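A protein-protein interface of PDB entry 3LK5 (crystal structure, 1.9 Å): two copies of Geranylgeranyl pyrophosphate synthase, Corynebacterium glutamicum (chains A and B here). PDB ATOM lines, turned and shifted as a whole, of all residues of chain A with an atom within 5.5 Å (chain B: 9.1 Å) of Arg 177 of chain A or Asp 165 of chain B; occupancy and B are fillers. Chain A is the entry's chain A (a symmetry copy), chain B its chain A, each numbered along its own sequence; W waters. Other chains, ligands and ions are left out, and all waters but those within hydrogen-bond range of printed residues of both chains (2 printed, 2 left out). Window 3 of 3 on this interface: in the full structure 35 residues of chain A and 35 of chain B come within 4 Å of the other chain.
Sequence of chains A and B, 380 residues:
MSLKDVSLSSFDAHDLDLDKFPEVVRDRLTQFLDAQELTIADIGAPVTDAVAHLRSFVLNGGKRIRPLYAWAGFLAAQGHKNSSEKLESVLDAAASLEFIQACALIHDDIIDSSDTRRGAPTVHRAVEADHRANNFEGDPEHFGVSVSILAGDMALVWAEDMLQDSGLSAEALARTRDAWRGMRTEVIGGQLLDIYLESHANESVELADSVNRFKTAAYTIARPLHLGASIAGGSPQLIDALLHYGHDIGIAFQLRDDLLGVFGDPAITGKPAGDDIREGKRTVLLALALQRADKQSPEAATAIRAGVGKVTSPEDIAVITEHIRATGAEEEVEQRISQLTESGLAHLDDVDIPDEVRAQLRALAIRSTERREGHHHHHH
Arg 177 of chain A touches just these residues of chain B: Asp 161 (2.9 Å), Gln 164 (3.5 Å) and Asp 165 (2.8 Å).
No residue of chain B comes within 4 Å of Thr 176 of chain A.
Printed residues of chain A within 4 Å of Asp 161 of chain B: Arg 177, Arg 181 and Arg 184.
Of the printed residues of chain A, Gln 164 of chain B touches Gln 164 (3.8 Å) and Arg 177 (3.5 Å).
Leu 173 of chain B touches none of the printed residues of chain A.
The nearest residue of chain B that does not touch Arg 177 of chain A is Glu 160 of chain B (4.9 Å).
The nearest printed residue of chain A that does not touch Asp 165 of chain B is Asp 178 of chain A (6.5 Å).
The nearest printed residue of chain B that does not touch Gln 164 of chain A is Glu 160 of chain B (6.2 Å).
O of Val 157 of chain B is in hydrogen-bond range of NH2 of Arg 184 of chain A, 3.1 Å away.
The guanidinium group (NH2) of Arg 177 of chain A lies within salt-bridge range of the side-chain carboxylate (OD1) of Asp 161 of chain B (2.9 Å).
OD1 of Asp 161 of chain B lies within salt-bridge range of NH1 of Arg 184 of chain A.
OD1 of Asp 165 of chain B is in salt-bridge range of NE of Arg 177 of chain A (2.8 Å).
The guanidinium group of Arg 181 of chain A is in salt-bridge range of the side-chain carboxylate of Asp 165 of chain B (2.9 Å).
Gln 164 of chain A touches its own counterpart, Gln 164 of chain B.
Positions printed for both chains: 164 and 173.
Of the 9 pairs that touch across the chains among the printed residues, 1 has its exchanged pair printed and touching as well.
Of the 12 printed residues of chain A, 4 touch a printed residue of chain B.
Printed residues of chain A that touch a printed residue of chain B: Gln 164, Arg 177, Arg 181 and Arg 184.
Of the 24 printed residues of chain B, 5 touch a printed residue of chain A.
Printed residues of chain B that touch a printed residue of chain A: Val 157, Glu 160, Asp 161, Gln 164 and Asp 165.
Among the printed residues, Asp or Glu carboxylates within 4 Å of a Lys or Arg side-chain nitrogen of the other chain: Arg 177 of chain A with Asp 161 of chain B (2.9 Å), Arg 177 of chain A with Asp 165 of chain B (2.8 Å), Arg 181 of chain A with Asp 165 of chain B (2.9 Å) and Arg 184 of chain A with Asp 161 of chain B (2.9 Å).
OD1 of Asp 178 of chain A is in salt-bridge range of NH1 of Arg 181 of chain A (3.1 Å).
The guanidinium group of Arg 184 of chain A is in hydrogen-bond range of the backbone carbonyl oxygen of Trp 180 of chain A (3.1 Å).
Water W2 lies within hydrogen-bond range of the backbone carbonyl oxygen (O) of Arg 181 of chain A, the side-chain carboxylate (OD2) of Asp 161 of chain B and the guanidinium group (NH1) of Arg 184 of chain A.
Water W1 lies within hydrogen-bond range of the guanidinium group of Arg 177 of chain A (2.8 Å), the guanidinium group of Arg 184 of chain A (3.2 Å) and the side-chain carboxylate of Asp 161 of chain B (3.4 Å).
OE1 of Gln 164 of chain A touches OE1 of Gln 164 of chain B (3.8 Å).
Gln 164 of chain B touches Arg 177 of chain A.
Arg 181 of chain A touches Asp 161 of chain B (CG to OD2, 3.8 Å).
NH2 of Arg 184 of chain A touches CB of Glu 160 of chain B, 3.5 Å away.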
ATOM      1  N   GLN A 164       5.193 -29.534  21.812  1.00  0.00           N
ATOM      2  CA  GLN A 164       5.519 -30.830  21.189  1.00  0.00           C
ATOM      3  C   GLN A 164       6.162 -31.774  22.220  1.00  0.00           C
ATOM      4  O   GLN A 164       6.000 -32.991  22.104  1.00  0.00           O
ATOM      5  CB  GLN A 164       6.504 -30.661  20.029  1.00  0.00           C
ATOM      6  CG  GLN A 164       5.889 -29.854  18.818  1.00  0.00           C
ATOM      7  CD  GLN A 164       4.544 -30.372  18.362  1.00  0.00           C
ATOM      8  OE1 GLN A 164       4.300 -31.573  18.362  1.00  0.00           O
ATOM      9  NE2 GLN A 164       3.661 -29.450  17.943  1.00  0.00           N
ATOM     10  N   LEU A 173      -1.810 -34.537  20.224  1.00  0.00           N
ATOM     11  CA  LEU A 173      -1.039 -33.590  19.386  1.00  0.00           C
ATOM     12  C   LEU A 173      -1.661 -33.375  18.032  1.00  0.00           C
ATOM     13  O   LEU A 173      -1.806 -32.236  17.590  1.00  0.00           O
ATOM     14  CB  LEU A 173       0.456 -34.004  19.239  1.00  0.00           C
ATOM     15  CG  LEU A 173       1.271 -33.815  20.500  1.00  0.00           C
ATOM     16  CD1 LEU A 173       2.642 -34.483  20.351  1.00  0.00           C
ATOM     17  CD2 LEU A 173       1.394 -32.295  20.844  1.00  0.00           C
ATOM     18  N   ALA A 174      -2.074 -34.465  17.385  1.00  0.00           N
ATOM     19  CA  ALA A 174      -2.735 -34.340  16.112  1.00  0.00           C
ATOM     20  C   ALA A 174      -4.001 -33.499  16.218  1.00  0.00           C
ATOM     21  O   ALA A 174      -4.306 -32.716  15.298  1.00  0.00           O
ATOM     22  CB  ALA A 174      -3.066 -35.740  15.498  1.00  0.00           C
ATOM     23  N   ARG A 175      -4.749 -33.662  17.322  1.00  0.00           N
ATOM     24  CA  ARG A 175      -6.002 -32.920  17.468  1.00  0.00           C
ATOM     25  C   ARG A 175      -5.737 -31.419  17.622  1.00  0.00           C
ATOM     26  O   ARG A 175      -6.591 -30.627  17.246  1.00  0.00           O
ATOM     27  CB  ARG A 175      -6.838 -33.418  18.676  1.00  0.00           C
ATOM     28  CG  ARG A 175      -7.566 -34.775  18.419  1.00  0.00           C
ATOM     29  CD  ARG A 175      -8.659 -35.072  19.494  1.00  0.00           C
ATOM     30  NE  ARG A 175      -8.097 -35.108  20.844  1.00  0.00           N
ATOM     31  CZ  ARG A 175      -7.599 -36.208  21.418  1.00  0.00           C
ATOM     32  NH1 ARG A 175      -7.108 -36.159  22.667  1.00  0.00           N
ATOM     33  NH2 ARG A 175      -7.588 -37.366  20.754  1.00  0.00           N
ATOM     34  N   THR A 176      -4.581 -31.057  18.171  1.00  0.00           N
ATOM     35  CA  THR A 176      -4.220 -29.635  18.373  1.00  0.00           C
ATOM     36  C   THR A 176      -4.006 -28.869  17.058  1.00  0.00           C
ATOM     37  O   THR A 176      -4.040 -27.644  17.074  1.00  0.00           O
ATOM     38  CB  THR A 176      -2.952 -29.404  19.243  1.00  0.00           C
ATOM     39  OG1 THR A 176      -1.762 -29.878  18.570  1.00  0.00           O
ATOM     40  CG2 THR A 176      -3.079 -30.065  20.638  1.00  0.00           C
ATOM     41  N   ARG A 177      -3.834 -29.565  15.935  1.00  0.00           N
ATOM     42  CA  ARG A 177      -3.335 -28.868  14.725  1.00  0.00           C
ATOM     43  C   ARG A 177      -4.224 -27.693  14.288  1.00  0.00           C
ATOM     44  O   ARG A 177      -3.729 -26.577  14.086  1.00  0.00           O
ATOM     45  CB  ARG A 177      -3.139 -29.847  13.548  1.00  0.00           C
ATOM     46  CG  ARG A 177      -1.987 -30.884  13.688  1.00  0.00           C
ATOM     47  CD  ARG A 177      -0.661 -30.181  13.944  1.00  0.00           C
ATOM     48  NE  ARG A 177      -0.356 -29.148  12.926  1.00  0.00           N
ATOM     49  CZ  ARG A 177       0.382 -28.076  13.199  1.00  0.00           C
ATOM     50  NH1 ARG A 177       0.839 -27.894  14.453  1.00  0.00           N
ATOM     51  NH2 ARG A 177       0.627 -27.173  12.239  1.00  0.00           N
ATOM     52  N   ASP A 178      -5.546 -27.922  14.171  1.00  0.00           N
ATOM     53  CA  ASP A 178      -6.425 -26.870  13.617  1.00  0.00           C
ATOM     54  C   ASP A 178      -6.338 -25.587  14.453  1.00  0.00           C
ATOM     55  O   ASP A 178      -6.169 -24.477  13.911  1.00  0.00           O
ATOM     56  CB  ASP A 178      -7.892 -27.338  13.492  1.00  0.00           C
ATOM     57  CG  ASP A 178      -8.092 -28.384  12.386  1.00  0.00           C
ATOM     58  OD1 ASP A 178      -7.222 -28.512  11.500  1.00  0.00           O
ATOM     59  OD2 ASP A 178      -9.135 -29.083  12.369  1.00  0.00           O
ATOM     60  N   ALA A 179      -6.455 -25.721  15.773  1.00  0.00           N
ATOM     61  CA  ALA A 179      -6.420 -24.553  16.620  1.00  0.00           C
ATOM     62  C   ALA A 179      -5.050 -23.905  16.624  1.00  0.00           C
ATOM     63  O   ALA A 179      -4.941 -22.678  16.580  1.00  0.00           O
ATOM     64  CB  ALA A 179      -6.825 -24.912  18.088  1.00  0.00           C
ATOM     65  N   TRP A 180      -4.000 -24.725  16.706  1.00  0.00           N
ATOM     66  CA  TRP A 180      -2.651 -24.165  16.823  1.00  0.00           C
ATOM     67  C   TRP A 180      -2.165 -23.568  15.500  1.00  0.00           C
ATOM     68  O   TRP A 180      -1.540 -22.466  15.495  1.00  0.00           O
ATOM     69  CB  TRP A 180      -1.688 -25.296  17.241  1.00  0.00           C
ATOM     70  CG  TRP A 180      -0.271 -24.870  17.613  1.00  0.00           C
ATOM     71  CD1 TRP A 180       0.840 -24.955  16.825  1.00  0.00           C
ATOM     72  CD2 TRP A 180       0.175 -24.420  18.898  1.00  0.00           C
ATOM     73  NE1 TRP A 180       1.961 -24.557  17.537  1.00  0.00           N
ATOM     74  CE2 TRP A 180       1.572 -24.206  18.806  1.00  0.00           C
ATOM     75  CE3 TRP A 180      -0.486 -24.181  20.127  1.00  0.00           C
ATOM     76  CZ2 TRP A 180       2.359 -23.769  19.909  1.00  0.00           C
ATOM     77  CZ3 TRP A 180       0.281 -23.754  21.242  1.00  0.00           C
ATOM     78  CH2 TRP A 180       1.690 -23.543  21.114  1.00  0.00           C
ATOM     79  N   ARG A 181      -2.440 -24.265  14.393  1.00  0.00           N
ATOM     80  CA  ARG A 181      -2.115 -23.704  13.056  1.00  0.00           C
ATOM     81  C   ARG A 181      -2.915 -22.383  12.858  1.00  0.00           C
ATOM     82  O   ARG A 181      -2.334 -21.352  12.486  1.00  0.00           O
ATOM     83  CB  ARG A 181      -2.478 -24.708  11.950  1.00  0.00           C
ATOM     84  CG  ARG A 181      -2.138 -24.235  10.496  1.00  0.00           C
ATOM     85  CD  ARG A 181      -2.971 -25.083   9.440  1.00  0.00           C
ATOM     86  NE  ARG A 181      -2.789 -26.503   9.734  1.00  0.00           N
ATOM     87  CZ  ARG A 181      -3.786 -27.325  10.046  1.00  0.00           C
ATOM     88  NH1 ARG A 181      -5.066 -26.910  10.032  1.00  0.00           N
ATOM     89  NH2 ARG A 181      -3.500 -28.558  10.322  1.00  0.00           N
ATOM     90  N   GLY A 182      -4.218 -22.426  13.169  1.00  0.00           N
ATOM     91  CA  GLY A 182      -5.087 -21.212  12.992  1.00  0.00           C
ATOM     92  C   GLY A 182      -4.564 -20.046  13.819  1.00  0.00           C
ATOM     93  O   GLY A 182      -4.309 -18.960  13.291  1.00  0.00           O
ATOM     94  N   ARG A 184      -1.672 -19.171  15.204  1.00  0.00           N
ATOM     95  CA  ARG A 184      -0.370 -18.511  14.932  1.00  0.00           C
ATOM     96  C   ARG A 184      -0.416 -17.752  13.607  1.00  0.00           C
ATOM     97  O   ARG A 184       0.133 -16.659  13.495  1.00  0.00           O
ATOM     98  CB  ARG A 184       0.801 -19.543  14.992  1.00  0.00           C
ATOM     99  CG  ARG A 184       1.090 -19.871  16.487  1.00  0.00           C
ATOM    100  CD  ARG A 184       1.380 -21.377  16.720  1.00  0.00           C
ATOM    101  NE  ARG A 184       2.519 -21.872  15.914  1.00  0.00           N
ATOM    102  CZ  ARG A 184       2.423 -22.569  14.777  1.00  0.00           C
ATOM    103  NH1 ARG A 184       1.236 -22.845  14.209  1.00  0.00           N
ATOM    104  NH2 ARG A 184       3.555 -23.029  14.206  1.00  0.00           N
ATOM    105  N   ARG B  28       7.951 -28.100  -3.461  1.00  0.00           N
ATOM    106  CA  ARG B  28       7.263 -28.318  -2.169  1.00  0.00           C
ATOM    107  C   ARG B  28       6.866 -26.982  -1.515  1.00  0.00           C
ATOM    108  O   ARG B  28       5.771 -26.858  -0.955  1.00  0.00           O
ATOM    109  CB  ARG B  28       8.161 -29.127  -1.192  1.00  0.00           C
ATOM    110  CG  ARG B  28       8.689 -30.486  -1.751  1.00  0.00           C
ATOM    111  CD  ARG B  28       7.591 -31.356  -2.415  1.00  0.00           C
ATOM    112  NE  ARG B  28       6.441 -31.645  -1.557  1.00  0.00           N
ATOM    113  CZ  ARG B  28       5.348 -32.281  -1.978  1.00  0.00           C
ATOM    114  NH1 ARG B  28       5.264 -32.691  -3.254  1.00  0.00           N
ATOM    115  NH2 ARG B  28       4.342 -32.509  -1.147  1.00  0.00           N
ATOM    116  N   PHE B  32       3.078 -25.411  -0.570  1.00  0.00           N
ATOM    117  CA  PHE B  32       2.725 -24.980   0.788  1.00  0.00           C
ATOM    118  C   PHE B  32       2.198 -23.540   0.766  1.00  0.00           C
ATOM    119  O   PHE B  32       1.162 -23.225   1.388  1.00  0.00           O
ATOM    120  CB  PHE B  32       3.962 -25.111   1.710  1.00  0.00           C
ATOM    121  CG  PHE B  32       3.688 -24.646   3.133  1.00  0.00           C
ATOM    122  CD1 PHE B  32       3.852 -23.311   3.489  1.00  0.00           C
ATOM    123  CD2 PHE B  32       3.240 -25.556   4.088  1.00  0.00           C
ATOM    124  CE1 PHE B  32       3.558 -22.863   4.817  1.00  0.00           C
ATOM    125  CE2 PHE B  32       2.952 -25.143   5.432  1.00  0.00           C
ATOM    126  CZ  PHE B  32       3.120 -23.799   5.797  1.00  0.00           C
ATOM    127  N   GLN B  36      -1.756 -21.548   1.656  1.00  0.00           N
ATOM    128  CA  GLN B  36      -2.025 -20.516   2.679  1.00  0.00           C
ATOM    129  C   GLN B  36      -2.807 -19.325   2.129  1.00  0.00           C
ATOM    130  O   GLN B  36      -3.245 -18.483   2.901  1.00  0.00           O
ATOM    131  CB  GLN B  36      -0.713 -19.957   3.267  1.00  0.00           C
ATOM    132  CG  GLN B  36       0.413 -21.006   3.652  1.00  0.00           C
ATOM    133  CD  GLN B  36      -0.075 -22.181   4.500  1.00  0.00           C
ATOM    134  OE1 GLN B  36      -0.635 -21.974   5.576  1.00  0.00           O
ATOM    135  NE2 GLN B  36       0.096 -23.440   3.983  1.00  0.00           N
ATOM    136  N   LYS B  86       5.643 -41.637   3.585  1.00  0.00           N
ATOM    137  CA  LYS B  86       5.386 -41.120   2.234  1.00  0.00           C
ATOM    138  C   LYS B  86       6.523 -40.232   1.791  1.00  0.00           C
ATOM    139  O   LYS B  86       6.987 -39.366   2.552  1.00  0.00           O
ATOM    140  CB  LYS B  86       4.060 -40.311   2.166  1.00  0.00           C
ATOM    141  CG  LYS B  86       2.810 -41.129   2.515  1.00  0.00           C
ATOM    142  CD  LYS B  86       1.504 -40.319   2.359  1.00  0.00           C
ATOM    143  CE  LYS B  86       1.330 -39.270   3.492  1.00  0.00           C
ATOM    144  NZ  LYS B  86       0.085 -38.423   3.299  1.00  0.00           N
ATOM    145  N   GLU B  88       6.500 -37.679  -0.250  1.00  0.00           N
ATOM    146  CA  GLU B  88       6.095 -36.287  -0.214  1.00  0.00           C
ATOM    147  C   GLU B  88       6.275 -35.699   1.201  1.00  0.00           C
ATOM    148  O   GLU B  88       6.608 -34.499   1.370  1.00  0.00           O
ATOM    149  CB  GLU B  88       4.601 -36.212  -0.589  1.00  0.00           C
ATOM    150  CG  GLU B  88       4.279 -36.742  -1.993  1.00  0.00           C
ATOM    151  CD  GLU B  88       4.319 -38.304  -2.166  1.00  0.00           C
ATOM    152  OE1 GLU B  88       4.389 -39.111  -1.209  1.00  0.00           O
ATOM    153  OE2 GLU B  88       4.237 -38.717  -3.352  1.00  0.00           O
ATOM    154  N   SER B  89       5.987 -36.517   2.206  1.00  0.00           N
ATOM    155  CA  SER B  89       6.105 -36.058   3.624  1.00  0.00           C
ATOM    156  C   SER B  89       7.555 -35.846   4.010  1.00  0.00           C
ATOM    157  O   SER B  89       7.888 -34.892   4.718  1.00  0.00           O
ATOM    158  CB  SER B  89       5.457 -37.065   4.580  1.00  0.00           C
ATOM    159  OG  SER B  89       4.080 -37.272   4.248  1.00  0.00           O
ATOM    160  N   VAL B  90       8.414 -36.764   3.578  1.00  0.00           N
ATOM    161  CA  VAL B  90       9.847 -36.577   3.822  1.00  0.00           C
ATOM    162  C   VAL B  90      10.353 -35.330   3.155  1.00  0.00           C
ATOM    163  O   VAL B  90      11.127 -34.539   3.765  1.00  0.00           O
ATOM    164  CB  VAL B  90      10.657 -37.826   3.353  1.00  0.00           C
ATOM    165  CG1 VAL B  90      12.155 -37.604   3.559  1.00  0.00           C
ATOM    166  CG2 VAL B  90      10.156 -39.067   4.092  1.00  0.00           C
ATOM    167  N   ASP B  92       8.662 -32.680   2.297  1.00  0.00           N
ATOM    168  CA  ASP B  92       8.124 -31.482   2.968  1.00  0.00           C
ATOM    169  C   ASP B  92       8.855 -31.188   4.258  1.00  0.00           C
ATOM    170  O   ASP B  92       9.130 -30.003   4.565  1.00  0.00           O
ATOM    171  CB  ASP B  92       6.643 -31.669   3.262  1.00  0.00           C
ATOM    172  CG  ASP B  92       5.772 -31.393   2.035  1.00  0.00           C
ATOM    173  OD1 ASP B  92       6.208 -30.790   1.045  1.00  0.00           O
ATOM    174  OD2 ASP B  92       4.631 -31.814   2.050  1.00  0.00           O
ATOM    175  N   ALA B  93       9.182 -32.260   5.008  1.00  0.00           N
ATOM    176  CA  ALA B  93      10.028 -32.066   6.218  1.00  0.00           C
ATOM    177  C   ALA B  93      11.355 -31.437   5.875  1.00  0.00           C
ATOM    178  O   ALA B  93      11.783 -30.485   6.544  1.00  0.00           O
ATOM    179  CB  ALA B  93      10.234 -33.401   6.992  1.00  0.00           C
ATOM    180  N   SER B  96      10.887 -27.720   4.802  1.00  0.00           N
ATOM    181  CA  SER B  96      10.454 -26.787   5.875  1.00  0.00           C
ATOM    182  C   SER B  96      11.658 -25.979   6.407  1.00  0.00           C
ATOM    183  O   SER B  96      11.503 -24.861   6.909  1.00  0.00           O
ATOM    184  CB  SER B  96       9.774 -27.540   7.033  1.00  0.00           C
ATOM    185  OG  SER B  96      10.762 -28.255   7.776  1.00  0.00           O
ATOM    186  N   VAL B 157       6.725 -19.713  12.034  1.00  0.00           N
ATOM    187  CA  VAL B 157       5.542 -20.523  12.340  1.00  0.00           C
ATOM    188  C   VAL B 157       5.200 -21.476  11.183  1.00  0.00           C
ATOM    189  O   VAL B 157       4.812 -22.617  11.416  1.00  0.00           O
ATOM    190  CB  VAL B 157       4.269 -19.712  12.867  1.00  0.00           C
ATOM    191  CG1 VAL B 157       4.634 -18.898  14.122  1.00  0.00           C
ATOM    192  CG2 VAL B 157       3.656 -18.882  11.853  1.00  0.00           C
ATOM    193  N   TRP B 158       5.437 -21.040   9.965  1.00  0.00           N
ATOM    194  CA  TRP B 158       5.151 -21.931   8.827  1.00  0.00           C
ATOM    195  C   TRP B 158       6.191 -23.060   8.680  1.00  0.00           C
ATOM    196  O   TRP B 158       5.858 -24.119   8.156  1.00  0.00           O
ATOM    197  CB  TRP B 158       5.056 -21.110   7.531  1.00  0.00           C
ATOM    198  CG  TRP B 158       3.715 -20.396   7.469  1.00  0.00           C
ATOM    199  CD1 TRP B 158       2.646 -20.546   8.330  1.00  0.00           C
ATOM    200  CD2 TRP B 158       3.300 -19.473   6.462  1.00  0.00           C
ATOM    201  NE1 TRP B 158       1.591 -19.702   7.929  1.00  0.00           N
ATOM    202  CE2 TRP B 158       1.981 -19.065   6.773  1.00  0.00           C
ATOM    203  CE3 TRP B 158       3.942 -18.923   5.329  1.00  0.00           C
ATOM    204  CZ2 TRP B 158       1.284 -18.143   5.986  1.00  0.00           C
ATOM    205  CZ3 TRP B 158       3.254 -17.992   4.551  1.00  0.00           C
ATOM    206  CH2 TRP B 158       1.936 -17.620   4.881  1.00  0.00           C
ATOM    207  N   ALA B 159       7.437 -22.808   9.086  1.00  0.00           N
ATOM    208  CA  ALA B 159       8.425 -23.923   9.150  1.00  0.00           C
ATOM    209  C   ALA B 159       7.860 -25.030  10.023  1.00  0.00           C
ATOM    210  O   ALA B 159       7.884 -26.232   9.663  1.00  0.00           O
ATOM    211  CB  ALA B 159       9.792 -23.455   9.694  1.00  0.00           C
ATOM    212  N   GLU B 160       7.349 -24.642  11.202  1.00  0.00           N
ATOM    213  CA  GLU B 160       6.825 -25.630  12.141  1.00  0.00           C
ATOM    214  C   GLU B 160       5.614 -26.311  11.527  1.00  0.00           C
ATOM    215  O   GLU B 160       5.486 -27.512  11.642  1.00  0.00           O
ATOM    216  CB  GLU B 160       6.398 -24.986  13.498  1.00  0.00           C
ATOM    217  CG  GLU B 160       7.454 -24.014  14.012  1.00  0.00           C
ATOM    218  CD  GLU B 160       8.629 -24.647  14.810  1.00  0.00           C
ATOM    219  OE1 GLU B 160       8.619 -25.950  14.921  1.00  0.00           O
ATOM    220  OE2 GLU B 160       9.510 -23.804  15.350  1.00  0.00           O
ATOM    221  N   ASP B 161       4.678 -25.528  10.968  1.00  0.00           N
ATOM    222  CA  ASP B 161       3.453 -26.129  10.363  1.00  0.00           C
ATOM    223  C   ASP B 161       3.843 -27.093   9.247  1.00  0.00           C
ATOM    224  O   ASP B 161       3.214 -28.132   9.080  1.00  0.00           O
ATOM    225  CB  ASP B 161       2.583 -25.040   9.734  1.00  0.00           C
ATOM    226  CG  ASP B 161       1.886 -24.154  10.789  1.00  0.00           C
ATOM    227  OD1 ASP B 161       1.759 -24.545  11.972  1.00  0.00           O
ATOM    228  OD2 ASP B 161       1.494 -23.043  10.426  1.00  0.00           O
ATOM    229  N   MET B 162       4.789 -26.691   8.419  1.00  0.00           N
ATOM    230  CA  MET B 162       5.134 -27.512   7.243  1.00  0.00           C
ATOM    231  C   MET B 162       5.659 -28.859   7.691  1.00  0.00           C
ATOM    232  O   MET B 162       5.327 -29.890   7.077  1.00  0.00           O
ATOM    233  CB  MET B 162       6.168 -26.801   6.350  1.00  0.00           C
ATOM    234  CG  MET B 162       6.370 -27.545   5.002  1.00  0.00           C
ATOM    235  SD  MET B 162       7.329 -26.365   3.787  1.00  0.00           S
ATOM    236  CE  MET B 162       7.344 -27.551   2.144  1.00  0.00           C
ATOM    237  N   LEU B 163       6.449 -28.870   8.773  1.00  0.00           N
ATOM    238  CA  LEU B 163       6.853 -30.135   9.392  1.00  0.00           C
ATOM    239  C   LEU B 163       5.662 -30.899  10.023  1.00  0.00           C
ATOM    240  O   LEU B 163       5.437 -32.090   9.711  1.00  0.00           O
ATOM    241  CB  LEU B 163       7.978 -29.905  10.456  1.00  0.00           C
ATOM    242  CG  LEU B 163       8.418 -31.193  11.196  1.00  0.00           C
ATOM    243  CD1 LEU B 163       9.070 -32.203  10.204  1.00  0.00           C
ATOM    244  CD2 LEU B 163       9.352 -30.845  12.373  1.00  0.00           C
ATOM    245  N   GLN B 164       4.900 -30.240  10.906  1.00  0.00           N
ATOM    246  CA  GLN B 164       3.873 -30.962  11.679  1.00  0.00           C
ATOM    247  C   GLN B 164       2.739 -31.434  10.753  1.00  0.00           C
ATOM    248  O   GLN B 164       2.121 -32.464  11.035  1.00  0.00           O
ATOM    249  CB  GLN B 164       3.257 -30.071  12.761  1.00  0.00           C
ATOM    250  CG  GLN B 164       4.293 -29.665  13.882  1.00  0.00           C
ATOM    251  CD  GLN B 164       5.052 -30.837  14.462  1.00  0.00           C
ATOM    252  OE1 GLN B 164       4.503 -31.920  14.632  1.00  0.00           O
ATOM    253  NE2 GLN B 164       6.332 -30.610  14.797  1.00  0.00           N
ATOM    254  N   ASP B 165       2.530 -30.724   9.650  1.00  0.00           N
ATOM    255  CA  ASP B 165       1.443 -31.047   8.694  1.00  0.00           C
ATOM    256  C   ASP B 165       1.903 -31.810   7.462  1.00  0.00           C
ATOM    257  O   ASP B 165       1.121 -32.005   6.505  1.00  0.00           O
ATOM    258  CB  ASP B 165       0.675 -29.791   8.250  1.00  0.00           C
ATOM    259  CG  ASP B 165      -0.166 -29.183   9.392  1.00  0.00           C
ATOM    260  OD1 ASP B 165      -0.686 -29.903  10.276  1.00  0.00           O
ATOM    261  OD2 ASP B 165      -0.260 -27.946   9.431  1.00  0.00           O
ATOM    262  N   SER B 166       3.155 -32.272   7.507  1.00  0.00           N
ATOM    263  CA  SER B 166       3.818 -32.911   6.359  1.00  0.00           C
ATOM    264  C   SER B 166       3.159 -34.234   5.984  1.00  0.00           C
ATOM    265  O   SER B 166       3.286 -34.682   4.834  1.00  0.00           O
ATOM    266  CB  SER B 166       5.286 -33.188   6.694  1.00  0.00           C
ATOM    267  OG  SER B 166       5.385 -34.010   7.855  1.00  0.00           O
ATOM    268  N   GLY B 167       2.510 -34.868   6.960  1.00  0.00           N
ATOM    269  CA  GLY B 167       1.976 -36.218   6.770  1.00  0.00           C
ATOM    270  C   GLY B 167       2.945 -37.291   7.237  1.00  0.00           C
ATOM    271  O   GLY B 167       2.646 -38.467   7.078  1.00  0.00           O
ATOM    272  N   LEU B 168       4.111 -36.911   7.802  1.00  0.00           N
ATOM    273  CA  LEU B 168       4.947 -37.881   8.551  1.00  0.00           C
ATOM    274  C   LEU B 168       4.077 -38.546   9.625  1.00  0.00           C
ATOM    275  O   LEU B 168       3.219 -37.882  10.230  1.00  0.00           O
ATOM    276  CB  LEU B 168       6.135 -37.179   9.237  1.00  0.00           C
ATOM    277  CG  LEU B 168       7.282 -36.722   8.306  1.00  0.00           C
ATOM    278  CD1 LEU B 168       8.377 -36.043   9.125  1.00  0.00           C
ATOM    279  CD2 LEU B 168       7.864 -37.936   7.547  1.00  0.00           C
ATOM    280  N   SER B 169       4.301 -39.832   9.849  1.00  0.00           N
ATOM    281  CA  SER B 169       3.616 -40.590  10.887  1.00  0.00           C
ATOM    282  C   SER B 169       3.919 -39.991  12.268  1.00  0.00           C
ATOM    283  O   SER B 169       4.934 -39.302  12.449  1.00  0.00           O
ATOM    284  CB  SER B 169       4.074 -42.049  10.854  1.00  0.00           C
ATOM    285  OG  SER B 169       5.437 -42.173  11.267  1.00  0.00           O
ATOM    286  N   LEU B 173       7.392 -38.232  13.456  1.00  0.00           N
ATOM    287  CA  LEU B 173       7.408 -36.911  14.126  1.00  0.00           C
ATOM    288  C   LEU B 173       8.091 -36.950  15.467  1.00  0.00           C
ATOM    289  O   LEU B 173       8.928 -36.097  15.762  1.00  0.00           O
ATOM    290  CB  LEU B 173       5.985 -36.291  14.258  1.00  0.00           C
ATOM    291  CG  LEU B 173       5.403 -35.808  12.947  1.00  0.00           C
ATOM    292  CD1 LEU B 173       3.920 -35.462  13.120  1.00  0.00           C
ATOM    293  CD2 LEU B 173       6.228 -34.598  12.401  1.00  0.00           C
HETATM  294  O   HOH W   1       3.087 -26.201  14.631  1.00  0.00           O
HETATM  295  O   HOH W   2       0.221 -20.995  11.675  1.00  0.00           O
